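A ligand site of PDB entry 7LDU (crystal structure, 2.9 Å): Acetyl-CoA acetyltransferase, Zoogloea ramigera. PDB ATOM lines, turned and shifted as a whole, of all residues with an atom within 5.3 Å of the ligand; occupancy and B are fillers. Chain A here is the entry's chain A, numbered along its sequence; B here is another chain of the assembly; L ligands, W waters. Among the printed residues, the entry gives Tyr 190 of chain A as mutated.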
ATOM      1  N   SCY A  96       5.475  25.150 -13.261  1.00  0.00           N
ATOM      2  CA  SCY A  96       5.194  24.646 -14.590  1.00  0.00           C
ATOM      3  CB  SCY A  96       5.100  23.135 -14.605  1.00  0.00           C
ATOM      4  SG  SCY A  96       6.635  22.371 -14.120  1.00  0.00           S
ATOM      5  CD  SCY A  96       6.640  22.327 -12.413  1.00  0.00           C
ATOM      6  OCD SCY A  96       5.693  22.529 -11.645  1.00  0.00           O
ATOM      7  CE  SCY A  96       8.006  22.018 -11.903  1.00  0.00           C
ATOM      8  C   SCY A  96       3.873  25.199 -15.249  1.00  0.00           C
ATOM      9  O   SCY A  96       3.701  25.053 -16.492  1.00  0.00           O
ATOM     10  N   LEU A 155      13.016  22.250  -9.515  1.00  0.00           N
ATOM     11  CA  LEU A 155      12.833  20.815  -9.676  1.00  0.00           C
ATOM     12  C   LEU A 155      12.835  20.034  -8.365  1.00  0.00           C
ATOM     13  O   LEU A 155      12.904  18.807  -8.389  1.00  0.00           O
ATOM     14  CB  LEU A 155      13.900  20.235 -10.607  1.00  0.00           C
ATOM     15  CG  LEU A 155      14.042  20.909 -11.977  1.00  0.00           C
ATOM     16  CD1 LEU A 155      15.203  20.322 -12.756  1.00  0.00           C
ATOM     17  CD2 LEU A 155      12.746  20.802 -12.766  1.00  0.00           C
ATOM     18  N   HIS A 163      13.360  15.037  -5.672  1.00  0.00           N
ATOM     19  CA  HIS A 163      13.164  15.596  -7.007  1.00  0.00           C
ATOM     20  C   HIS A 163      11.716  15.432  -7.452  1.00  0.00           C
ATOM     21  O   HIS A 163      10.943  14.662  -6.884  1.00  0.00           O
ATOM     22  CB  HIS A 163      14.110  14.936  -8.009  1.00  0.00           C
ATOM     23  CG  HIS A 163      14.427  15.790  -9.198  1.00  0.00           C
ATOM     24  ND1 HIS A 163      13.592  15.883 -10.287  1.00  0.00           N
ATOM     25  CD2 HIS A 163      15.501  16.566  -9.477  1.00  0.00           C
ATOM     26  CE1 HIS A 163      14.124  16.699 -11.178  1.00  0.00           C
ATOM     27  NE2 HIS A 163      15.287  17.128 -10.714  1.00  0.00           N
ATOM     28  N   MET A 164      11.363  16.188  -8.490  1.00  0.00           N
ATOM     29  CA  MET A 164      10.034  16.055  -9.082  1.00  0.00           C
ATOM     30  C   MET A 164       9.814  14.677  -9.687  1.00  0.00           C
ATOM     31  O   MET A 164       8.673  14.226  -9.800  1.00  0.00           O
ATOM     32  CB  MET A 164       9.826  17.151 -10.129  1.00  0.00           C
ATOM     33  CG  MET A 164       9.903  18.554  -9.562  1.00  0.00           C
ATOM     34  SD  MET A 164       8.441  19.014  -8.629  1.00  0.00           S
ATOM     35  CE  MET A 164       7.210  18.906  -9.915  1.00  0.00           C
ATOM     36  N   GLY A 165      10.895  14.006 -10.099  1.00  0.00           N
ATOM     37  CA  GLY A 165      10.764  12.662 -10.633  1.00  0.00           C
ATOM     38  C   GLY A 165      10.258  11.662  -9.616  1.00  0.00           C
ATOM     39  O   GLY A 165       9.640  10.662  -9.972  1.00  0.00           O
ATOM     40  N   TYR A 190       7.382  10.414 -28.932  1.00  0.00           N
ATOM     41  CA  TYR A 190       8.453  10.729 -29.876  1.00  0.00           C
ATOM     42  C   TYR A 190       7.992  10.523 -31.315  1.00  0.00           C
ATOM     43  O   TYR A 190       8.349  11.304 -32.204  1.00  0.00           O
ATOM     44  CB  TYR A 190       9.690   9.874 -29.581  1.00  0.00           C
ATOM     45  CG  TYR A 190      10.503  10.341 -28.400  1.00  0.00           C
ATOM     46  CD1 TYR A 190      11.406  11.396 -28.533  1.00  0.00           C
ATOM     47  CD2 TYR A 190      10.383   9.738 -27.164  1.00  0.00           C
ATOM     48  CE1 TYR A 190      12.160  11.827 -27.468  1.00  0.00           C
ATOM     49  CE2 TYR A 190      11.143  10.165 -26.077  1.00  0.00           C
ATOM     50  CZ  TYR A 190      12.026  11.206 -26.236  1.00  0.00           C
ATOM     51  OH  TYR A 190      12.780  11.637 -25.171  1.00  0.00           O
ATOM     52  N   ARG A 227      13.937  13.524 -31.348  1.00  0.00           N
ATOM     53  CA  ARG A 227      14.824  12.455 -31.785  1.00  0.00           C
ATOM     54  C   ARG A 227      14.014  11.198 -32.055  1.00  0.00           C
ATOM     55  O   ARG A 227      12.805  11.130 -31.779  1.00  0.00           O
ATOM     56  CB  ARG A 227      15.890  12.171 -30.722  1.00  0.00           C
ATOM     57  CG  ARG A 227      15.278  11.707 -29.416  1.00  0.00           C
ATOM     58  CD  ARG A 227      16.300  11.389 -28.333  1.00  0.00           C
ATOM     59  NE  ARG A 227      17.062  10.185 -28.611  1.00  0.00           N
ATOM     60  CZ  ARG A 227      18.209   9.862 -28.014  1.00  0.00           C
ATOM     61  NH1 ARG A 227      18.737  10.667 -27.105  1.00  0.00           N
ATOM     62  NH2 ARG A 227      18.830   8.734 -28.336  1.00  0.00           N
ATOM     63  N   ALA A 229      13.396   7.520 -30.978  1.00  0.00           N
ATOM     64  CA  ALA A 229      13.570   6.609 -29.855  1.00  0.00           C
ATOM     65  C   ALA A 229      13.130   5.201 -30.221  1.00  0.00           C
ATOM     66  O   ALA A 229      12.225   5.001 -31.037  1.00  0.00           O
ATOM     67  CB  ALA A 229      12.772   7.100 -28.638  1.00  0.00           C
ATOM     68  N   SER A 233      16.201   0.712 -26.935  1.00  0.00           N
ATOM     69  CA  SER A 233      17.101   1.753 -26.475  1.00  0.00           C
ATOM     70  C   SER A 233      16.525   2.531 -25.297  1.00  0.00           C
ATOM     71  O   SER A 233      17.264   3.300 -24.663  1.00  0.00           O
ATOM     72  CB  SER A 233      17.423   2.714 -27.616  1.00  0.00           C
ATOM     73  OG  SER A 233      18.373   3.691 -27.222  1.00  0.00           O
ATOM     74  N   MET A 234      15.248   2.339 -24.981  1.00  0.00           N
ATOM     75  CA  MET A 234      14.613   2.978 -23.834  1.00  0.00           C
ATOM     76  C   MET A 234      14.488   2.052 -22.640  1.00  0.00           C
ATOM     77  O   MET A 234      14.395   2.544 -21.502  1.00  0.00           O
ATOM     78  CB  MET A 234      13.219   3.486 -24.224  1.00  0.00           C
ATOM     79  CG  MET A 234      12.644   4.525 -23.274  1.00  0.00           C
ATOM     80  SD  MET A 234      12.849   6.205 -23.900  1.00  0.00           S
ATOM     81  CE  MET A 234      11.702   6.202 -25.275  1.00  0.00           C
ATOM     82  N   LEU A 237      17.782   2.108 -20.242  1.00  0.00           N
ATOM     83  CA  LEU A 237      18.124   3.297 -19.470  1.00  0.00           C
ATOM     84  C   LEU A 237      17.902   3.039 -17.987  1.00  0.00           C
ATOM     85  O   LEU A 237      16.885   2.464 -17.591  1.00  0.00           O
ATOM     86  CB  LEU A 237      17.280   4.486 -19.927  1.00  0.00           C
ATOM     87  CG  LEU A 237      17.394   4.870 -21.403  1.00  0.00           C
ATOM     88  CD1 LEU A 237      16.519   6.081 -21.722  1.00  0.00           C
ATOM     89  CD2 LEU A 237      18.839   5.145 -21.781  1.00  0.00           C
ATOM     90  N   ALA A 240      16.845   7.473 -13.080  1.00  0.00           N
ATOM     91  CA  ALA A 240      17.675   8.599 -12.691  1.00  0.00           C
ATOM     92  C   ALA A 240      17.314   9.165 -11.318  1.00  0.00           C
ATOM     93  O   ALA A 240      18.074   9.982 -10.789  1.00  0.00           O
ATOM     94  CB  ALA A 240      17.567   9.724 -13.736  1.00  0.00           C
ATOM     95  N   PHE A 241      16.193   8.746 -10.739  1.00  0.00           N
ATOM     96  CA  PHE A 241      15.721   9.285  -9.471  1.00  0.00           C
ATOM     97  C   PHE A 241      15.778   8.294  -8.326  1.00  0.00           C
ATOM     98  O   PHE A 241      16.101   8.677  -7.200  1.00  0.00           O
ATOM     99  CB  PHE A 241      14.287   9.808  -9.634  1.00  0.00           C
ATOM    100  CG  PHE A 241      14.132  10.834 -10.715  1.00  0.00           C
ATOM    101  CD1 PHE A 241      14.476  12.156 -10.497  1.00  0.00           C
ATOM    102  CD2 PHE A 241      13.660  10.467 -11.973  1.00  0.00           C
ATOM    103  CE1 PHE A 241      14.347  13.095 -11.497  1.00  0.00           C
ATOM    104  CE2 PHE A 241      13.531  11.406 -12.973  1.00  0.00           C
ATOM    105  CZ  PHE A 241      13.871  12.727 -12.735  1.00  0.00           C
ATOM    106  N   THR A 248      12.841   7.077 -15.955  1.00  0.00           N
ATOM    107  CA  THR A 248      14.171   7.201 -16.519  1.00  0.00           C
ATOM    108  C   THR A 248      14.294   8.531 -17.258  1.00  0.00           C
ATOM    109  O   THR A 248      13.353   9.327 -17.310  1.00  0.00           O
ATOM    110  CB  THR A 248      14.484   6.033 -17.461  1.00  0.00           C
ATOM    111  OG1 THR A 248      13.677   6.130 -18.636  1.00  0.00           O
ATOM    112  CG2 THR A 248      14.204   4.711 -16.765  1.00  0.00           C
ATOM    113  N   ALA A 249      15.474   8.771 -17.826  1.00  0.00           N
ATOM    114  CA  ALA A 249      15.691   9.991 -18.592  1.00  0.00           C
ATOM    115  C   ALA A 249      14.930   9.991 -19.907  1.00  0.00           C
ATOM    116  O   ALA A 249      14.779  11.049 -20.535  1.00  0.00           O
ATOM    117  CB  ALA A 249      17.182  10.202 -18.852  1.00  0.00           C
ATOM    118  N   GLY A 250      14.447   8.826 -20.349  1.00  0.00           N
ATOM    119  CA  GLY A 250      13.724   8.728 -21.601  1.00  0.00           C
ATOM    120  C   GLY A 250      12.227   8.931 -21.449  1.00  0.00           C
ATOM    121  O   GLY A 250      11.611   9.656 -22.246  1.00  0.00           O
ATOM    122  N   ALA A 252      10.850  10.607 -19.191  1.00  0.00           N
ATOM    123  CA  ALA A 252      10.647  11.846 -18.458  1.00  0.00           C
ATOM    124  C   ALA A 252      11.083  13.021 -19.335  1.00  0.00           C
ATOM    125  O   ALA A 252      12.025  12.905 -20.129  1.00  0.00           O
ATOM    126  CB  ALA A 252      11.435  11.872 -17.146  1.00  0.00           C
ATOM    127  N   SER A 253      10.387  14.141 -19.172  1.00  0.00           N
ATOM    128  CA  SER A 253      10.740  15.339 -19.912  1.00  0.00           C
ATOM    129  C   SER A 253      12.113  15.849 -19.470  1.00  0.00           C
ATOM    130  O   SER A 253      12.535  15.643 -18.331  1.00  0.00           O
ATOM    131  CB  SER A 253       9.682  16.429 -19.703  1.00  0.00           C
ATOM    132  OG  SER A 253       9.522  16.736 -18.335  1.00  0.00           O
ATOM    133  N   GLY A 254      12.805  16.520 -20.388  1.00  0.00           N
ATOM    134  CA  GLY A 254      14.138  17.017 -20.130  1.00  0.00           C
ATOM    135  C   GLY A 254      14.145  18.469 -19.687  1.00  0.00           C
ATOM    136  O   GLY A 254      13.111  19.100 -19.462  1.00  0.00           O
ATOM    137  N   LEU A 255      15.363  18.995 -19.553  1.00  0.00           N
ATOM    138  CA  LEU A 255      15.576  20.393 -19.214  1.00  0.00           C
ATOM    139  C   LEU A 255      15.759  21.174 -20.507  1.00  0.00           C
ATOM    140  O   LEU A 255      16.629  20.838 -21.310  1.00  0.00           O
ATOM    141  CB  LEU A 255      16.784  20.547 -18.297  1.00  0.00           C
ATOM    142  CG  LEU A 255      16.946  19.439 -17.240  1.00  0.00           C
ATOM    143  CD1 LEU A 255      18.271  19.587 -16.505  1.00  0.00           C
ATOM    144  CD2 LEU A 255      15.789  19.458 -16.262  1.00  0.00           C
ATOM    145  N   MET A 294       1.847  15.355  -7.228  1.00  0.00           N
ATOM    146  CA  MET A 294       1.569  16.586  -7.964  1.00  0.00           C
ATOM    147  C   MET A 294       1.178  16.323  -9.403  1.00  0.00           C
ATOM    148  O   MET A 294       0.563  17.184 -10.038  1.00  0.00           O
ATOM    149  CB  MET A 294       2.793  17.501  -7.926  1.00  0.00           C
ATOM    150  CG  MET A 294       3.975  16.984  -8.727  1.00  0.00           C
ATOM    151  SD  MET A 294       3.981  17.560 -10.439  1.00  0.00           S
ATOM    152  CE  MET A 294       5.032  16.338 -11.210  1.00  0.00           C
ATOM    153  N   ALA A 324       4.829  15.933 -18.299  1.00  0.00           N
ATOM    154  CA  ALA A 324       5.982  16.092 -17.414  1.00  0.00           C
ATOM    155  C   ALA A 324       6.699  14.765 -17.228  1.00  0.00           C
ATOM    156  O   ALA A 324       7.940  14.699 -17.291  1.00  0.00           O
ATOM    157  CB  ALA A 324       5.535  16.668 -16.068  1.00  0.00           C
ATOM    158  N   PHE A 325       5.939  13.698 -16.984  1.00  0.00           N
ATOM    159  CA  PHE A 325       6.471  12.359 -16.888  1.00  0.00           C
ATOM    160  C   PHE A 325       5.490  11.396 -17.533  1.00  0.00           C
ATOM    161  O   PHE A 325       4.297  11.688 -17.660  1.00  0.00           O
ATOM    162  CB  PHE A 325       6.742  11.946 -15.436  1.00  0.00           C
ATOM    163  CG  PHE A 325       7.693  12.845 -14.709  1.00  0.00           C
ATOM    164  CD1 PHE A 325       9.053  12.606 -14.738  1.00  0.00           C
ATOM    165  CD2 PHE A 325       7.227  13.936 -13.989  1.00  0.00           C
ATOM    166  CE1 PHE A 325       9.938  13.434 -14.081  1.00  0.00           C
ATOM    167  CE2 PHE A 325       8.110  14.764 -13.322  1.00  0.00           C
ATOM    168  CZ  PHE A 325       9.460  14.518 -13.363  1.00  0.00           C
ATOM    169  N   HIS A 354      10.576  20.579 -22.064  1.00  0.00           N
ATOM    170  CA  HIS A 354       9.822  21.101 -20.928  1.00  0.00           C
ATOM    171  C   HIS A 354      10.522  22.327 -20.345  1.00  0.00           C
ATOM    172  O   HIS A 354      11.134  22.252 -19.271  1.00  0.00           O
ATOM    173  CB  HIS A 354       9.643  20.025 -19.858  1.00  0.00           C
ATOM    174  CG  HIS A 354       8.561  20.324 -18.866  1.00  0.00           C
ATOM    175  ND1 HIS A 354       7.965  21.562 -18.757  1.00  0.00           N
ATOM    176  CD2 HIS A 354       7.965  19.538 -17.936  1.00  0.00           C
ATOM    177  CE1 HIS A 354       7.061  21.529 -17.801  1.00  0.00           C
ATOM    178  NE2 HIS A 354       7.041  20.315 -17.290  1.00  0.00           N
ATOM    179  N   ILE A 356      10.109  24.996 -18.069  1.00  0.00           N
ATOM    180  CA  ILE A 356       9.102  25.055 -17.005  1.00  0.00           C
ATOM    181  C   ILE A 356       8.265  26.329 -17.118  1.00  0.00           C
ATOM    182  O   ILE A 356       7.031  26.278 -17.235  1.00  0.00           O
ATOM    183  CB  ILE A 356       9.758  24.937 -15.618  1.00  0.00           C
ATOM    184  CG1 ILE A 356      11.122  25.639 -15.596  1.00  0.00           C
ATOM    185  CG2 ILE A 356       9.914  23.473 -15.240  1.00  0.00           C
ATOM    186  CD1 ILE A 356      11.825  25.546 -14.258  1.00  0.00           C
ATOM    187  N   CYS A 384       0.517  19.976 -15.159  1.00  0.00           N
ATOM    188  CA  CYS A 384       0.707  19.719 -13.744  1.00  0.00           C
ATOM    189  C   CYS A 384       1.737  20.690 -13.180  1.00  0.00           C
ATOM    190  O   CYS A 384       2.661  21.112 -13.872  1.00  0.00           O
ATOM    191  CB  CYS A 384       1.131  18.282 -13.482  1.00  0.00           C
ATOM    192  SG  CYS A 384       2.812  17.884 -14.008  1.00  0.00           S
ATOM    193  N   GLY A 386       4.310  21.794  -9.821  1.00  0.00           N
ATOM    194  CA  GLY A 386       5.010  21.349  -8.629  1.00  0.00           C
ATOM    195  C   GLY A 386       4.394  21.898  -7.361  1.00  0.00           C
ATOM    196  O   GLY A 386       3.726  22.935  -7.341  1.00  0.00           O
ATOM    197  N   MET B 141      25.100  19.878 -14.093  1.00  0.00           N
ATOM    198  CA  MET B 141      23.865  19.792 -13.322  1.00  0.00           C
ATOM    199  C   MET B 141      24.205  19.388 -11.895  1.00  0.00           C
ATOM    200  O   MET B 141      25.137  18.616 -11.659  1.00  0.00           O
ATOM    201  CB  MET B 141      22.892  18.795 -13.947  1.00  0.00           C
ATOM    202  CG  MET B 141      21.543  18.701 -13.251  1.00  0.00           C
ATOM    203  SD  MET B 141      20.436  17.548 -14.077  1.00  0.00           S
ATOM    204  CE  MET B 141      20.381  16.224 -12.864  1.00  0.00           C
HETATM  205  N1  LIG L   1      16.319   7.249 -25.700  1.00  0.00           N
HETATM  206  C1  LIG L   1      17.513   6.686 -25.539  1.00  0.00           C
HETATM  207  N2  LIG L   1      18.472   7.245 -24.833  1.00  0.00           N
HETATM  208  C2  LIG L   1      18.259   8.420 -24.239  1.00  0.00           C
HETATM  209  C3  LIG L   1      17.003   9.055 -24.377  1.00  0.00           C
HETATM  210  C4  LIG L   1      16.019   8.425 -25.144  1.00  0.00           C
HETATM  211  N3  LIG L   1      14.783   9.020 -25.322  1.00  0.00           N
HETATM  212  N4  LIG L   1      17.055  10.225 -23.697  1.00  0.00           N
HETATM  213  C5  LIG L   1      18.230  10.343 -23.138  1.00  0.00           C
HETATM  214  N5  LIG L   1      19.006   9.262 -23.445  1.00  0.00           N
HETATM  215  C6  LIG L   1      20.376   9.052 -23.000  1.00  0.00           C
HETATM  216  C7  LIG L   1      21.328  10.197 -23.495  1.00  0.00           C
HETATM  217  O1  LIG L   1      21.753  10.081 -24.868  1.00  0.00           O
HETATM  218  C8  LIG L   1      22.491   9.892 -22.526  1.00  0.00           C
HETATM  219  O2  LIG L   1      23.068   8.658 -22.915  1.00  0.00           O
HETATM  220  P1  LIG L   1      24.643   8.731 -22.644  1.00  0.00           P
HETATM  221  O3  LIG L   1      25.004  10.023 -22.005  1.00  0.00           O
HETATM  222  O4  LIG L   1      25.021   7.503 -21.663  1.00  0.00           O
HETATM  223  O5  LIG L   1      25.388   8.602 -24.064  1.00  0.00           O
HETATM  224  C9  LIG L   1      21.729   9.695 -21.203  1.00  0.00           C
HETATM  225  O6  LIG L   1      20.432   9.149 -21.549  1.00  0.00           O
HETATM  226  C10 LIG L   1      21.646  11.029 -20.438  1.00  0.00           C
HETATM  227  O7  LIG L   1      20.295  11.470 -20.210  1.00  0.00           O
HETATM  228  P2  LIG L   1      20.221  13.002 -20.710  1.00  0.00           P
HETATM  229  O8  LIG L   1      19.444  13.102 -21.981  1.00  0.00           O
HETATM  230  O9  LIG L   1      21.706  13.521 -21.053  1.00  0.00           O
HETATM  231  O10 LIG L   1      19.472  13.926 -19.598  1.00  0.00           O
HETATM  232  P3  LIG L   1      20.254  13.963 -18.185  1.00  0.00           P
HETATM  233  O11 LIG L   1      21.174  12.802 -18.037  1.00  0.00           O
HETATM  234  O12 LIG L   1      21.082  15.342 -18.128  1.00  0.00           O
HETATM  235  O13 LIG L   1      19.241  13.972 -16.931  1.00  0.00           O
HETATM  236  C11 LIG L   1      16.966  13.870 -16.214  1.00  0.00           C
HETATM  237  C12 LIG L   1      17.961  13.467 -17.312  1.00  0.00           C
HETATM  238  C13 LIG L   1      15.828  12.859 -16.106  1.00  0.00           C
HETATM  239  C14 LIG L   1      17.753  13.886 -14.903  1.00  0.00           C
HETATM  240  C15 LIG L   1      16.364  15.232 -16.568  1.00  0.00           C
HETATM  241  O14 LIG L   1      15.917  15.199 -17.922  1.00  0.00           O
HETATM  242  C16 LIG L   1      15.202  15.568 -15.663  1.00  0.00           C
HETATM  243  O15 LIG L   1      15.346  15.519 -14.459  1.00  0.00           O
HETATM  244  N6  LIG L   1      13.994  15.935 -16.157  1.00  0.00           N
HETATM  245  C17 LIG L   1      12.907  16.252 -15.226  1.00  0.00           C
HETATM  246  C18 LIG L   1      12.034  17.375 -15.775  1.00  0.00           C
HETATM  247  C19 LIG L   1      11.112  17.921 -14.714  1.00  0.00           C
HETATM  248  O16 LIG L   1      11.288  17.682 -13.536  1.00  0.00           O
HETATM  249  N7  LIG L   1      10.077  18.693 -15.125  1.00  0.00           N
HETATM  250  C20 LIG L   1       9.119  19.282 -14.202  1.00  0.00           C
HETATM  251  C21 LIG L   1       8.196  18.181 -13.697  1.00  0.00           C
HETATM  252  S1  LIG L   1       6.575  18.933 -13.423  1.00  0.00           S
HETATM  253  O   HOH W   1      17.217  16.591 -12.056  1.00  0.00           O
HETATM  254  O   HOH W   2      18.667  16.542 -19.638  1.00  0.00           O
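SG of SCY 96 lies close to NE2 of His 354, 3.8 Å away.
N of Gly 250 lies close to OG1 of Thr 248 (3.3 Å).
The backbone carbonyl oxygen (O) of Leu 155 is in hydrogen-bond range of the backbone NH (N) of Met 164 (3.0 Å).
A ring nitrogen (ND1) of His 163 lies close to the backbone NH (N) of Gly 165 (3.3 Å).
The side-chain hydroxyl of Ser 253 sits at hydrogen-bond distance from the backbone carbonyl oxygen of Ala 324 (2.8 Å).
SD of Met 294 lies within hydrogen-bond range of SG of Cys 384 (3.8 Å).
OCD of SCY 96 is in hydrogen-bond range of N of Gly 386 (2.4 Å).
The side-chain sulfur (SD) of Met 234 sits at hydrogen-bond distance from a nitrogen (N3) of the ligand (3.7 Å).
A nitrogen (N6) of the ligand lies within hydrogen-bond range of the backbone carbonyl oxygen (O) of Ser 253 (2.6 Å).
SG of SCY 96 sits close to a sulfur (S1) of the ligand, 3.5 Å away.
The side-chain hydroxyl (OH) of Tyr 190 lies within hydrogen-bond range of a nitrogen (N3) of the ligand.
Merely in contact with the ligand: Gly 254 (3.4 Å), Phe 325 (3.4 Å), Ser 233 (3.5 Å), Leu 155 (3.5 Å), Met 164 (3.6 Å), Phe 241 (3.6 Å), Arg 227 (3.6 Å), His 354 (3.6 Å), Ala 249 (3.6 Å), Ala 324 (3.6 Å), His 163 (3.7 Å), Leu 237 (3.7 Å), Met 294 (3.7 Å), Gly 250 (3.9 Å), Cys 384 (3.95 Å) and Leu 255 (3.96 Å).
Hydrophobic or aromatic side chains that line the ligand: Leu 155, His 163, Met 164, Tyr 190, Met 234, Leu 237, Phe 241, Ala 249, Leu 255, Met 294, Ala 324, Phe 325 and His 354.
Within 4 Å of the ligand: SCY 96, Leu 155, His 163, Met 164, Tyr 190, Arg 227, Ser 233, Met 234, Leu 237, Phe 241, Ala 249, Gly 250, Ser 253, Gly 254, Leu 255, Met 294, Ala 324, Phe 325, His 354 and Cys 384.
Water W1 lies within hydrogen-bond range of NE2 of His 163 (2.4 Å) and O15 of the ligand (3.2 Å).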
